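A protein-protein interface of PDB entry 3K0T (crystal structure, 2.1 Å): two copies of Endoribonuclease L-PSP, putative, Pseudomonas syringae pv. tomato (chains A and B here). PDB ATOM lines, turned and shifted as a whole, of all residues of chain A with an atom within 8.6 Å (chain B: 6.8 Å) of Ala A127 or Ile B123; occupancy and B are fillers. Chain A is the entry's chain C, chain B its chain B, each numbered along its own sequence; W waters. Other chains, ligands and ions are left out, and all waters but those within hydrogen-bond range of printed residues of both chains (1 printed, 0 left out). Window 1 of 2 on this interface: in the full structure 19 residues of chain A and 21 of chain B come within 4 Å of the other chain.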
ATOM      1  N   GLY A  49       9.196  24.311 -10.682  1.00  0.00           N
ATOM      2  CA  GLY A  49       8.644  25.346 -11.525  1.00  0.00           C
ATOM      3  C   GLY A  49       8.120  26.438 -10.613  1.00  0.00           C
ATOM      4  O   GLY A  49       7.575  26.158  -9.553  1.00  0.00           O
ATOM      5  N   ILE A  51       5.562  29.775 -10.323  1.00  0.00           N
ATOM      6  CA  ILE A  51       4.470  30.467 -10.971  1.00  0.00           C
ATOM      7  C   ILE A  51       4.453  31.875 -10.412  1.00  0.00           C
ATOM      8  O   ILE A  51       5.130  32.146  -9.396  1.00  0.00           O
ATOM      9  CB  ILE A  51       3.107  29.745 -10.879  1.00  0.00           C
ATOM     10  CG1 ILE A  51       2.760  29.365  -9.426  1.00  0.00           C
ATOM     11  CG2 ILE A  51       3.094  28.538 -11.821  1.00  0.00           C
ATOM     12  CD1 ILE A  51       1.289  28.851  -9.259  1.00  0.00           C
ATOM     13  N   ASN A  93      13.499  26.304 -18.430  1.00  0.00           N
ATOM     14  CA  ASN A  93      12.352  25.897 -19.245  1.00  0.00           C
ATOM     15  C   ASN A  93      11.252  26.938 -19.107  1.00  0.00           C
ATOM     16  O   ASN A  93      10.872  27.285 -17.988  1.00  0.00           O
ATOM     17  CB  ASN A  93      11.798  24.542 -18.791  1.00  0.00           C
ATOM     18  CG  ASN A  93      12.729  23.396 -19.108  1.00  0.00           C
ATOM     19  OD1 ASN A  93      13.100  22.618 -18.222  1.00  0.00           O
ATOM     20  ND2 ASN A  93      13.107  23.276 -20.375  1.00  0.00           N
ATOM     21  N   ILE A  94      10.742  27.427 -20.238  1.00  0.00           N
ATOM     22  CA  ILE A  94       9.670  28.423 -20.231  1.00  0.00           C
ATOM     23  C   ILE A  94       8.343  27.819 -20.722  1.00  0.00           C
ATOM     24  O   ILE A  94       8.259  27.278 -21.834  1.00  0.00           O
ATOM     25  CB  ILE A  94      10.025  29.651 -21.121  1.00  0.00           C
ATOM     26  CG1 ILE A  94      11.208  30.427 -20.522  1.00  0.00           C
ATOM     27  CG2 ILE A  94       8.817  30.568 -21.259  1.00  0.00           C
ATOM     28  CD1 ILE A  94      12.050  31.172 -21.564  1.00  0.00           C
ATOM     29  N   PHE A  95       7.318  27.916 -19.877  1.00  0.00           N
ATOM     30  CA  PHE A  95       5.982  27.421 -20.210  1.00  0.00           C
ATOM     31  C   PHE A  95       5.047  28.641 -20.261  1.00  0.00           C
ATOM     32  O   PHE A  95       4.898  29.371 -19.268  1.00  0.00           O
ATOM     33  CB  PHE A  95       5.491  26.414 -19.154  1.00  0.00           C
ATOM     34  CG  PHE A  95       6.503  25.334 -18.814  1.00  0.00           C
ATOM     35  CD1 PHE A  95       6.807  24.311 -19.718  1.00  0.00           C
ATOM     36  CD2 PHE A  95       7.155  25.352 -17.585  1.00  0.00           C
ATOM     37  CE1 PHE A  95       7.749  23.318 -19.393  1.00  0.00           C
ATOM     38  CE2 PHE A  95       8.097  24.369 -17.249  1.00  0.00           C
ATOM     39  CZ  PHE A  95       8.395  23.353 -18.153  1.00  0.00           C
ATOM     40  N   LEU A  96       4.447  28.870 -21.428  1.00  0.00           N
ATOM     41  CA  LEU A  96       3.525  29.989 -21.635  1.00  0.00           C
ATOM     42  C   LEU A  96       2.213  29.471 -22.219  1.00  0.00           C
ATOM     43  O   LEU A  96       2.211  28.593 -23.088  1.00  0.00           O
ATOM     44  CB  LEU A  96       4.122  31.016 -22.617  1.00  0.00           C
ATOM     45  CG  LEU A  96       5.312  31.905 -22.192  1.00  0.00           C
ATOM     46  CD1 LEU A  96       5.986  32.495 -23.426  1.00  0.00           C
ATOM     47  CD2 LEU A  96       4.851  33.021 -21.252  1.00  0.00           C
ATOM     48  N   THR A  97       1.095  29.988 -21.724  1.00  0.00           N
ATOM     49  CA  THR A  97      -0.195  29.605 -22.276  1.00  0.00           C
ATOM     50  C   THR A  97      -0.377  30.408 -23.561  1.00  0.00           C
ATOM     51  O   THR A  97      -1.135  30.020 -24.448  1.00  0.00           O
ATOM     52  CB  THR A  97      -1.356  29.914 -21.308  1.00  0.00           C
ATOM     53  OG1 THR A  97      -1.227  31.252 -20.808  1.00  0.00           O
ATOM     54  CG2 THR A  97      -1.370  28.916 -20.149  1.00  0.00           C
ATOM     55  N   ASP A  98       0.329  31.527 -23.672  1.00  0.00           N
ATOM     56  CA  ASP A  98       0.224  32.337 -24.884  1.00  0.00           C
ATOM     57  C   ASP A  98       1.618  32.748 -25.333  1.00  0.00           C
ATOM     58  O   ASP A  98       2.248  33.594 -24.716  1.00  0.00           O
ATOM     59  CB  ASP A  98      -0.628  33.580 -24.628  1.00  0.00           C
ATOM     60  CG  ASP A  98      -0.798  34.446 -25.868  1.00  0.00           C
ATOM     61  OD1 ASP A  98      -0.170  34.160 -26.916  1.00  0.00           O
ATOM     62  OD2 ASP A  98      -1.554  35.437 -25.789  1.00  0.00           O
ATOM     63  N   ILE A 123       7.866  26.342 -24.652  1.00  0.00           N
ATOM     64  CA  ILE A 123       6.705  25.723 -25.278  1.00  0.00           C
ATOM     65  C   ILE A 123       5.390  26.405 -24.891  1.00  0.00           C
ATOM     66  O   ILE A 123       5.277  27.021 -23.829  1.00  0.00           O
ATOM     67  CB  ILE A 123       6.587  24.195 -24.914  1.00  0.00           C
ATOM     68  CG1 ILE A 123       6.345  24.029 -23.416  1.00  0.00           C
ATOM     69  CG2 ILE A 123       7.856  23.434 -25.347  1.00  0.00           C
ATOM     70  CD1 ILE A 123       6.126  22.574 -22.943  1.00  0.00           C
ATOM     71  N   GLY A 124       4.401  26.275 -25.777  1.00  0.00           N
ATOM     72  CA  GLY A 124       3.069  26.801 -25.529  1.00  0.00           C
ATOM     73  C   GLY A 124       2.233  25.689 -24.911  1.00  0.00           C
ATOM     74  O   GLY A 124       2.024  24.645 -25.537  1.00  0.00           O
ATOM     75  N   VAL A 125       1.773  25.897 -23.680  1.00  0.00           N
ATOM     76  CA  VAL A 125       0.987  24.879 -22.991  1.00  0.00           C
ATOM     77  C   VAL A 125      -0.520  25.182 -23.032  1.00  0.00           C
ATOM     78  O   VAL A 125      -0.924  26.311 -23.297  1.00  0.00           O
ATOM     79  CB  VAL A 125       1.439  24.716 -21.517  1.00  0.00           C
ATOM     80  CG1 VAL A 125       2.909  24.310 -21.459  1.00  0.00           C
ATOM     81  CG2 VAL A 125       1.217  26.014 -20.736  1.00  0.00           C
ATOM     82  N   ALA A 126      -1.354  24.176 -22.783  1.00  0.00           N
ATOM     83  CA  ALA A 126      -2.798  24.389 -22.810  1.00  0.00           C
ATOM     84  C   ALA A 126      -3.275  25.130 -21.558  1.00  0.00           C
ATOM     85  O   ALA A 126      -4.214  25.924 -21.627  1.00  0.00           O
ATOM     86  CB  ALA A 126      -3.526  23.046 -22.938  1.00  0.00           C
ATOM     87  N   ALA A 127      -2.622  24.886 -20.423  1.00  0.00           N
ATOM     88  CA  ALA A 127      -3.007  25.519 -19.170  1.00  0.00           C
ATOM     89  C   ALA A 127      -1.895  25.427 -18.123  1.00  0.00           C
ATOM     90  O   ALA A 127      -1.028  24.562 -18.208  1.00  0.00           O
ATOM     91  CB  ALA A 127      -4.281  24.856 -18.634  1.00  0.00           C
ATOM     92  N   LEU A 128      -1.930  26.321 -17.136  1.00  0.00           N
ATOM     93  CA  LEU A 128      -0.942  26.323 -16.054  1.00  0.00           C
ATOM     94  C   LEU A 128      -1.639  26.323 -14.700  1.00  0.00           C
ATOM     95  O   LEU A 128      -2.791  26.747 -14.594  1.00  0.00           O
ATOM     96  CB  LEU A 128      -0.016  27.537 -16.184  1.00  0.00           C
ATOM     97  CG  LEU A 128       0.970  27.386 -17.350  1.00  0.00           C
ATOM     98  CD1 LEU A 128       1.711  28.695 -17.584  1.00  0.00           C
ATOM     99  CD2 LEU A 128       1.951  26.256 -17.044  1.00  0.00           C
ATOM    100  N   PRO A 129      -0.968  25.812 -13.657  1.00  0.00           N
ATOM    101  CA  PRO A 129      -1.585  25.787 -12.325  1.00  0.00           C
ATOM    102  C   PRO A 129      -2.098  27.179 -11.912  1.00  0.00           C
ATOM    103  O   PRO A 129      -1.455  28.197 -12.201  1.00  0.00           O
ATOM    104  CB  PRO A 129      -0.442  25.329 -11.424  1.00  0.00           C
ATOM    105  CG  PRO A 129       0.396  24.461 -12.327  1.00  0.00           C
ATOM    106  CD  PRO A 129       0.367  25.177 -13.653  1.00  0.00           C
ATOM    107  N   ARG A 130      -3.253  27.219 -11.252  1.00  0.00           N
ATOM    108  CA  ARG A 130      -3.852  28.470 -10.760  1.00  0.00           C
ATOM    109  C   ARG A 130      -4.272  29.486 -11.815  1.00  0.00           C
ATOM    110  O   ARG A 130      -4.718  30.581 -11.472  1.00  0.00           O
ATOM    111  CB  ARG A 130      -2.905  29.189  -9.783  1.00  0.00           C
ATOM    112  CG  ARG A 130      -2.338  28.326  -8.672  1.00  0.00           C
ATOM    113  CD  ARG A 130      -1.794  29.177  -7.503  1.00  0.00           C
ATOM    114  NE  ARG A 130      -1.117  28.313  -6.536  1.00  0.00           N
ATOM    115  CZ  ARG A 130      -1.175  28.450  -5.212  1.00  0.00           C
ATOM    116  NH1 ARG A 130      -1.888  29.427  -4.651  1.00  0.00           N
ATOM    117  NH2 ARG A 130      -0.511  27.600  -4.442  1.00  0.00           N
ATOM    118  N   GLY A 131      -4.138  29.142 -13.090  1.00  0.00           N
ATOM    119  CA  GLY A 131      -4.492  30.081 -14.145  1.00  0.00           C
ATOM    120  C   GLY A 131      -3.328  31.012 -14.467  1.00  0.00           C
ATOM    121  O   GLY A 131      -3.508  32.040 -15.116  1.00  0.00           O
ATOM    122  N   ALA A 132      -2.131  30.650 -14.021  1.00  0.00           N
ATOM    123  CA  ALA A 132      -0.940  31.455 -14.305  1.00  0.00           C
ATOM    124  C   ALA A 132      -0.710  31.534 -15.812  1.00  0.00           C
ATOM    125  O   ALA A 132      -1.045  30.608 -16.543  1.00  0.00           O
ATOM    126  CB  ALA A 132       0.289  30.837 -13.623  1.00  0.00           C
ATOM    127  N   GLN A 133      -0.141  32.637 -16.279  1.00  0.00           N
ATOM    128  CA  GLN A 133       0.134  32.784 -17.704  1.00  0.00           C
ATOM    129  C   GLN A 133       1.520  32.258 -18.025  1.00  0.00           C
ATOM    130  O   GLN A 133       1.841  31.977 -19.177  1.00  0.00           O
ATOM    131  CB  GLN A 133       0.112  34.245 -18.113  1.00  0.00           C
ATOM    132  CG  GLN A 133      -1.197  34.944 -17.951  1.00  0.00           C
ATOM    133  CD  GLN A 133      -1.031  36.397 -18.305  1.00  0.00           C
ATOM    134  OE1 GLN A 133      -1.496  36.850 -19.346  1.00  0.00           O
ATOM    135  NE2 GLN A 133      -0.308  37.135 -17.457  1.00  0.00           N
ATOM    136  N   VAL A 134       2.349  32.140 -16.999  1.00  0.00           N
ATOM    137  CA  VAL A 134       3.712  31.688 -17.209  1.00  0.00           C
ATOM    138  C   VAL A 134       4.212  30.848 -16.037  1.00  0.00           C
ATOM    139  O   VAL A 134       3.785  31.024 -14.898  1.00  0.00           O
ATOM    140  CB  VAL A 134       4.658  32.923 -17.475  1.00  0.00           C
ATOM    141  CG1 VAL A 134       4.589  33.926 -16.318  1.00  0.00           C
ATOM    142  CG2 VAL A 134       6.112  32.462 -17.709  1.00  0.00           C
ATOM    143  N   GLU A 135       5.068  29.882 -16.347  1.00  0.00           N
ATOM    144  CA  GLU A 135       5.715  29.047 -15.342  1.00  0.00           C
ATOM    145  C   GLU A 135       7.101  28.785 -15.897  1.00  0.00           C
ATOM    146  O   GLU A 135       7.274  28.678 -17.103  1.00  0.00           O
ATOM    147  CB  GLU A 135       4.992  27.706 -15.126  1.00  0.00           C
ATOM    148  CG  GLU A 135       5.710  26.759 -14.106  1.00  0.00           C
ATOM    149  CD  GLU A 135       5.000  25.418 -13.912  1.00  0.00           C
ATOM    150  OE1 GLU A 135       3.822  25.307 -14.312  1.00  0.00           O
ATOM    151  OE2 GLU A 135       5.607  24.468 -13.364  1.00  0.00           O
ATOM    152  N   MET A 136       8.085  28.707 -15.012  1.00  0.00           N
ATOM    153  CA  MET A 136       9.445  28.402 -15.433  1.00  0.00           C
ATOM    154  C   MET A 136      10.167  27.562 -14.385  1.00  0.00           C
ATOM    155  O   MET A 136       9.990  27.773 -13.188  1.00  0.00           O
ATOM    156  CB  MET A 136      10.275  29.685 -15.652  1.00  0.00           C
ATOM    157  CG  MET A 136       9.757  30.643 -16.696  1.00  0.00           C
ATOM    158  SD  MET A 136      10.983  32.157 -16.888  1.00  0.00           S
ATOM    159  CE  MET A 136       9.697  33.543 -17.250  1.00  0.00           C
ATOM    160  N   ASP A 137      10.949  26.584 -14.833  1.00  0.00           N
ATOM    161  CA  ASP A 137      11.786  25.850 -13.896  1.00  0.00           C
ATOM    162  C   ASP A 137      13.222  25.935 -14.395  1.00  0.00           C
ATOM    163  O   ASP A 137      13.473  26.409 -15.504  1.00  0.00           O
ATOM    164  CB  ASP A 137      11.314  24.407 -13.601  1.00  0.00           C
ATOM    165  CG  ASP A 137      11.463  23.443 -14.772  1.00  0.00           C
ATOM    166  OD1 ASP A 137      12.144  23.747 -15.769  1.00  0.00           O
ATOM    167  OD2 ASP A 137      10.885  22.345 -14.660  1.00  0.00           O
ATOM    168  N   ASN B  93       8.374  15.640 -13.164  1.00  0.00           N
ATOM    169  CA  ASN B  93       7.546  16.487 -14.000  1.00  0.00           C
ATOM    170  C   ASN B  93       6.149  15.892 -14.159  1.00  0.00           C
ATOM    171  O   ASN B  93       5.993  14.701 -14.436  1.00  0.00           O
ATOM    172  CB  ASN B  93       8.196  16.712 -15.376  1.00  0.00           C
ATOM    173  CG  ASN B  93       9.507  17.491 -15.285  1.00  0.00           C
ATOM    174  OD1 ASN B  93      10.563  16.995 -15.689  1.00  0.00           O
ATOM    175  ND2 ASN B  93       9.443  18.714 -14.756  1.00  0.00           N
ATOM    176  N   ILE B  94       5.137  16.734 -13.971  1.00  0.00           N
ATOM    177  CA  ILE B  94       3.760  16.296 -14.089  1.00  0.00           C
ATOM    178  C   ILE B  94       3.131  16.870 -15.346  1.00  0.00           C
ATOM    179  O   ILE B  94       3.092  18.091 -15.523  1.00  0.00           O
ATOM    180  CB  ILE B  94       2.918  16.741 -12.863  1.00  0.00           C
ATOM    181  CG1 ILE B  94       3.381  15.989 -11.602  1.00  0.00           C
ATOM    182  CG2 ILE B  94       1.432  16.469 -13.128  1.00  0.00           C
ATOM    183  CD1 ILE B  94       2.998  16.680 -10.272  1.00  0.00           C
ATOM    184  N   PHE B  95       2.655  15.990 -16.229  1.00  0.00           N
ATOM    185  CA  PHE B  95       1.983  16.440 -17.443  1.00  0.00           C
ATOM    186  C   PHE B  95       0.537  15.974 -17.366  1.00  0.00           C
ATOM    187  O   PHE B  95       0.266  14.776 -17.273  1.00  0.00           O
ATOM    188  CB  PHE B  95       2.662  15.879 -18.693  1.00  0.00           C
ATOM    189  CG  PHE B  95       4.146  16.162 -18.753  1.00  0.00           C
ATOM    190  CD1 PHE B  95       4.625  17.466 -18.885  1.00  0.00           C
ATOM    191  CD2 PHE B  95       5.060  15.120 -18.661  1.00  0.00           C
ATOM    192  CE1 PHE B  95       5.999  17.725 -18.927  1.00  0.00           C
ATOM    193  CE2 PHE B  95       6.434  15.368 -18.700  1.00  0.00           C
ATOM    194  CZ  PHE B  95       6.903  16.668 -18.833  1.00  0.00           C
ATOM    195  N   LEU B  96      -0.395  16.922 -17.398  1.00  0.00           N
ATOM    196  CA  LEU B  96      -1.810  16.578 -17.306  1.00  0.00           C
ATOM    197  C   LEU B  96      -2.599  17.193 -18.447  1.00  0.00           C
ATOM    198  O   LEU B  96      -2.390  18.354 -18.801  1.00  0.00           O
ATOM    199  CB  LEU B  96      -2.407  17.073 -15.979  1.00  0.00           C
ATOM    200  CG  LEU B  96      -2.147  16.385 -14.638  1.00  0.00           C
ATOM    201  CD1 LEU B  96      -2.691  17.257 -13.488  1.00  0.00           C
ATOM    202  CD2 LEU B  96      -2.823  15.008 -14.626  1.00  0.00           C
ATOM    203  N   THR B  97      -3.511  16.419 -19.030  1.00  0.00           N
ATOM    204  CA  THR B  97      -4.333  16.974 -20.096  1.00  0.00           C
ATOM    205  C   THR B  97      -5.373  17.908 -19.468  1.00  0.00           C
ATOM    206  O   THR B  97      -5.861  18.828 -20.123  1.00  0.00           O
ATOM    207  CB  THR B  97      -5.030  15.872 -20.945  1.00  0.00           C
ATOM    208  OG1 THR B  97      -5.609  14.889 -20.084  1.00  0.00           O
ATOM    209  CG2 THR B  97      -4.028  15.215 -21.877  1.00  0.00           C
ATOM    210  N   ASP B  98      -5.685  17.690 -18.192  1.00  0.00           N
ATOM    211  CA  ASP B  98      -6.661  18.528 -17.477  1.00  0.00           C
ATOM    212  C   ASP B  98      -6.176  18.789 -16.048  1.00  0.00           C
ATOM    213  O   ASP B  98      -6.052  17.856 -15.250  1.00  0.00           O
ATOM    214  CB  ASP B  98      -8.039  17.837 -17.423  1.00  0.00           C
ATOM    215  CG  ASP B  98      -9.151  18.780 -16.961  1.00  0.00           C
ATOM    216  OD1 ASP B  98      -8.866  19.723 -16.196  1.00  0.00           O
ATOM    217  OD2 ASP B  98     -10.317  18.575 -17.357  1.00  0.00           O
ATOM    218  N   LEU B  99      -5.909  20.053 -15.718  1.00  0.00           N
ATOM    219  CA  LEU B  99      -5.429  20.394 -14.374  1.00  0.00           C
ATOM    220  C   LEU B  99      -6.546  20.324 -13.336  1.00  0.00           C
ATOM    221  O   LEU B  99      -6.321  20.530 -12.145  1.00  0.00           O
ATOM    222  CB  LEU B  99      -4.773  21.773 -14.368  1.00  0.00           C
ATOM    223  CG  LEU B  99      -3.449  21.853 -15.139  1.00  0.00           C
ATOM    224  CD1 LEU B  99      -2.971  23.293 -15.159  1.00  0.00           C
ATOM    225  CD2 LEU B  99      -2.392  20.930 -14.495  1.00  0.00           C
ATOM    226  N   ALA B 121       7.640  20.203 -11.395  1.00  0.00           N
ATOM    227  CA  ALA B 121       7.009  21.147 -12.303  1.00  0.00           C
ATOM    228  C   ALA B 121       5.686  20.493 -12.677  1.00  0.00           C
ATOM    229  O   ALA B 121       5.541  19.274 -12.563  1.00  0.00           O
ATOM    230  CB  ALA B 121       7.873  21.352 -13.552  1.00  0.00           C
ATOM    231  N   ALA B 122       4.723  21.290 -13.107  1.00  0.00           N
ATOM    232  CA  ALA B 122       3.433  20.742 -13.499  1.00  0.00           C
ATOM    233  C   ALA B 122       2.815  21.662 -14.522  1.00  0.00           C
ATOM    234  O   ALA B 122       2.691  22.869 -14.286  1.00  0.00           O
ATOM    235  CB  ALA B 122       2.507  20.603 -12.282  1.00  0.00           C
ATOM    236  N   ILE B 123       2.447  21.094 -15.668  1.00  0.00           N
ATOM    237  CA  ILE B 123       1.823  21.865 -16.731  1.00  0.00           C
ATOM    238  C   ILE B 123       0.628  21.128 -17.329  1.00  0.00           C
ATOM    239  O   ILE B 123       0.559  19.903 -17.295  1.00  0.00           O
ATOM    240  CB  ILE B 123       2.825  22.194 -17.893  1.00  0.00           C
ATOM    241  CG1 ILE B 123       3.370  20.904 -18.523  1.00  0.00           C
ATOM    242  CG2 ILE B 123       3.969  23.075 -17.364  1.00  0.00           C
ATOM    243  CD1 ILE B 123       4.256  21.128 -19.782  1.00  0.00           C
ATOM    244  N   GLY B 124      -0.306  21.905 -17.867  1.00  0.00           N
ATOM    245  CA  GLY B 124      -1.464  21.352 -18.545  1.00  0.00           C
ATOM    246  C   GLY B 124      -1.087  21.257 -20.011  1.00  0.00           C
ATOM    247  O   GLY B 124      -0.724  22.261 -20.625  1.00  0.00           O
ATOM    248  N   VAL B 125      -1.146  20.047 -20.564  1.00  0.00           N
ATOM    249  CA  VAL B 125      -0.777  19.814 -21.957  1.00  0.00           C
ATOM    250  C   VAL B 125      -2.022  19.604 -22.815  1.00  0.00           C
ATOM    251  O   VAL B 125      -3.116  19.383 -22.282  1.00  0.00           O
ATOM    252  CB  VAL B 125       0.160  18.574 -22.092  1.00  0.00           C
ATOM    253  CG1 VAL B 125       1.368  18.741 -21.189  1.00  0.00           C
ATOM    254  CG2 VAL B 125      -0.579  17.289 -21.711  1.00  0.00           C
ATOM    255  N   ALA B 126      -1.854  19.687 -24.136  1.00  0.00           N
ATOM    256  CA  ALA B 126      -2.960  19.517 -25.076  1.00  0.00           C
ATOM    257  C   ALA B 126      -3.298  18.035 -25.211  1.00  0.00           C
ATOM    258  O   ALA B 126      -4.471  17.662 -25.302  1.00  0.00           O
ATOM    259  CB  ALA B 126      -2.589  20.104 -26.443  1.00  0.00           C
HETATM  260  O   HOH W   1      10.609  20.605 -16.615  1.00  0.00           O
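Among the printed residues, merely in contact across the chains: Pro A129 with Ala B122 (3.3 Å), Leu A128 with Leu B99 (3.3 Å), Asp A137 with Ala B121 (3.4 Å), Val A125 with Gly B124 (3.4 Å), Pro A129 with Leu B99 (3.6 Å), Phe A95 with Ile B123 (3.7 Å), Ala A126 with Val B125 (3.7 Å), Glu A135 with Ala B121 (3.8 Å), Leu A128 with Ile B123 (3.8 Å), Glu A135 with Ile B123 (3.8 Å), Ala A127 with Leu B99 (3.8 Å), Val A125 with Ile B123 (3.8 Å), Asp A137 with Asn B93 (3.9 Å), Ala A127 with Ile B123 (3.9 Å), Ala A126 with Ala B126 (3.9 Å) and Ile A123 with Ile B123 (3.9 Å).
Phe A95 touches Ile B123, but with the chains exchanged Ile A123 does not touch Phe B95 (6.3 Å). Ile A123 touches its own counterpart, Ile B123. Val A125 touches Gly B124, but with the chains exchanged Gly A124 does not touch Val B125 (6.6 Å). Ala A126 touches Val B125, but with the chains exchanged Val A125 does not touch Ala B126 (5.8 Å). Of the 19 pairs that touch across the chains among the printed residues, 2 have their exchanged pair printed and touching as well.
Of the printed residues of chain B, Ile A123 touches Ile B123 (3.9 Å). Ala A127 touches three residues of chain B. Of the printed residues of chain B, Leu A128 touches Leu B99 (3.3 Å) and Ile B123 (3.8 Å). Of the printed residues of chain B, Pro A129 touches Leu B99 (3.6 Å) and Ala B122 (3.3 Å). Printed residues of chain A within 4 Å of Asn B93: Asp A137. Ala B122 touches two residues of chain A. Of chain A, only Phe A95 (3.7 Å), Ile A123 (3.9 Å), Val A125 (3.8 Å), Ala A127 (3.9 Å), Leu A128 (3.8 Å) and Glu A135 (3.8 Å) come within 4 Å of Ile B123. Gly B124 touches just these residues of chain A: Val A125, Ala A126 and Ala A127. Printed residues of chain A within 4 Å of Ala B126: Ala A126. The nearest residue of chain A that does not touch Ile B123 is Pro A129 (4.8 Å). The nearest printed residue of chain B that does not touch Val A125 is Val B125 (5.4 Å).
O of Ile B123 sits at hydrogen-bond distance from N of Leu B96, 3.1 Å away. The backbone carbonyl oxygen (O) of Ile A123 is in hydrogen-bond range of the backbone NH (N) of Leu A96, 3.1 Å away. O of Leu A96 sits at hydrogen-bond distance from N of Val A125 (2.8 Å). O of Ile B94 is in hydrogen-bond range of N of Ile B123, 3.1 Å away. OD1 of Asn A93 lies close to OD1 of Asp A137 (2.9 Å). The backbone carbonyl oxygen (O) of Glu A135 lies within hydrogen-bond range of the backbone NH (N) of Phe A95 (2.9 Å).
N of Ala B122 is in hydrogen-bond range of OE2 of Glu A135 (3.3 Å). N of Gly B124 is in hydrogen-bond range of O of Ala A127 (2.8 Å). The backbone carbonyl oxygen (O) of Gly B124 sits at hydrogen-bond distance from the backbone NH (N) of Ala A126.
Hydrophobic or aromatic side chains of chain B within 4 Å of the printed part of chain A: Leu B99, Ala B121 and Ile B123. Hydrophobic or aromatic side chains of chain A within 4 Å of the printed part of chain B: Phe A95, Ile A123, Val A125, Ala A126, Leu A128 and Pro A129. Among the printed residues, 19 pairs touch across the chains. Among the printed residues, no Asp or Glu carboxylate lies within 4 Å of a Lys or Arg side-chain nitrogen of the other chain.
Water W1 lies within hydrogen-bond range of OD2 of Asp A137 (2.6 Å) and ND2 of Asn B93 (2.9 Å).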
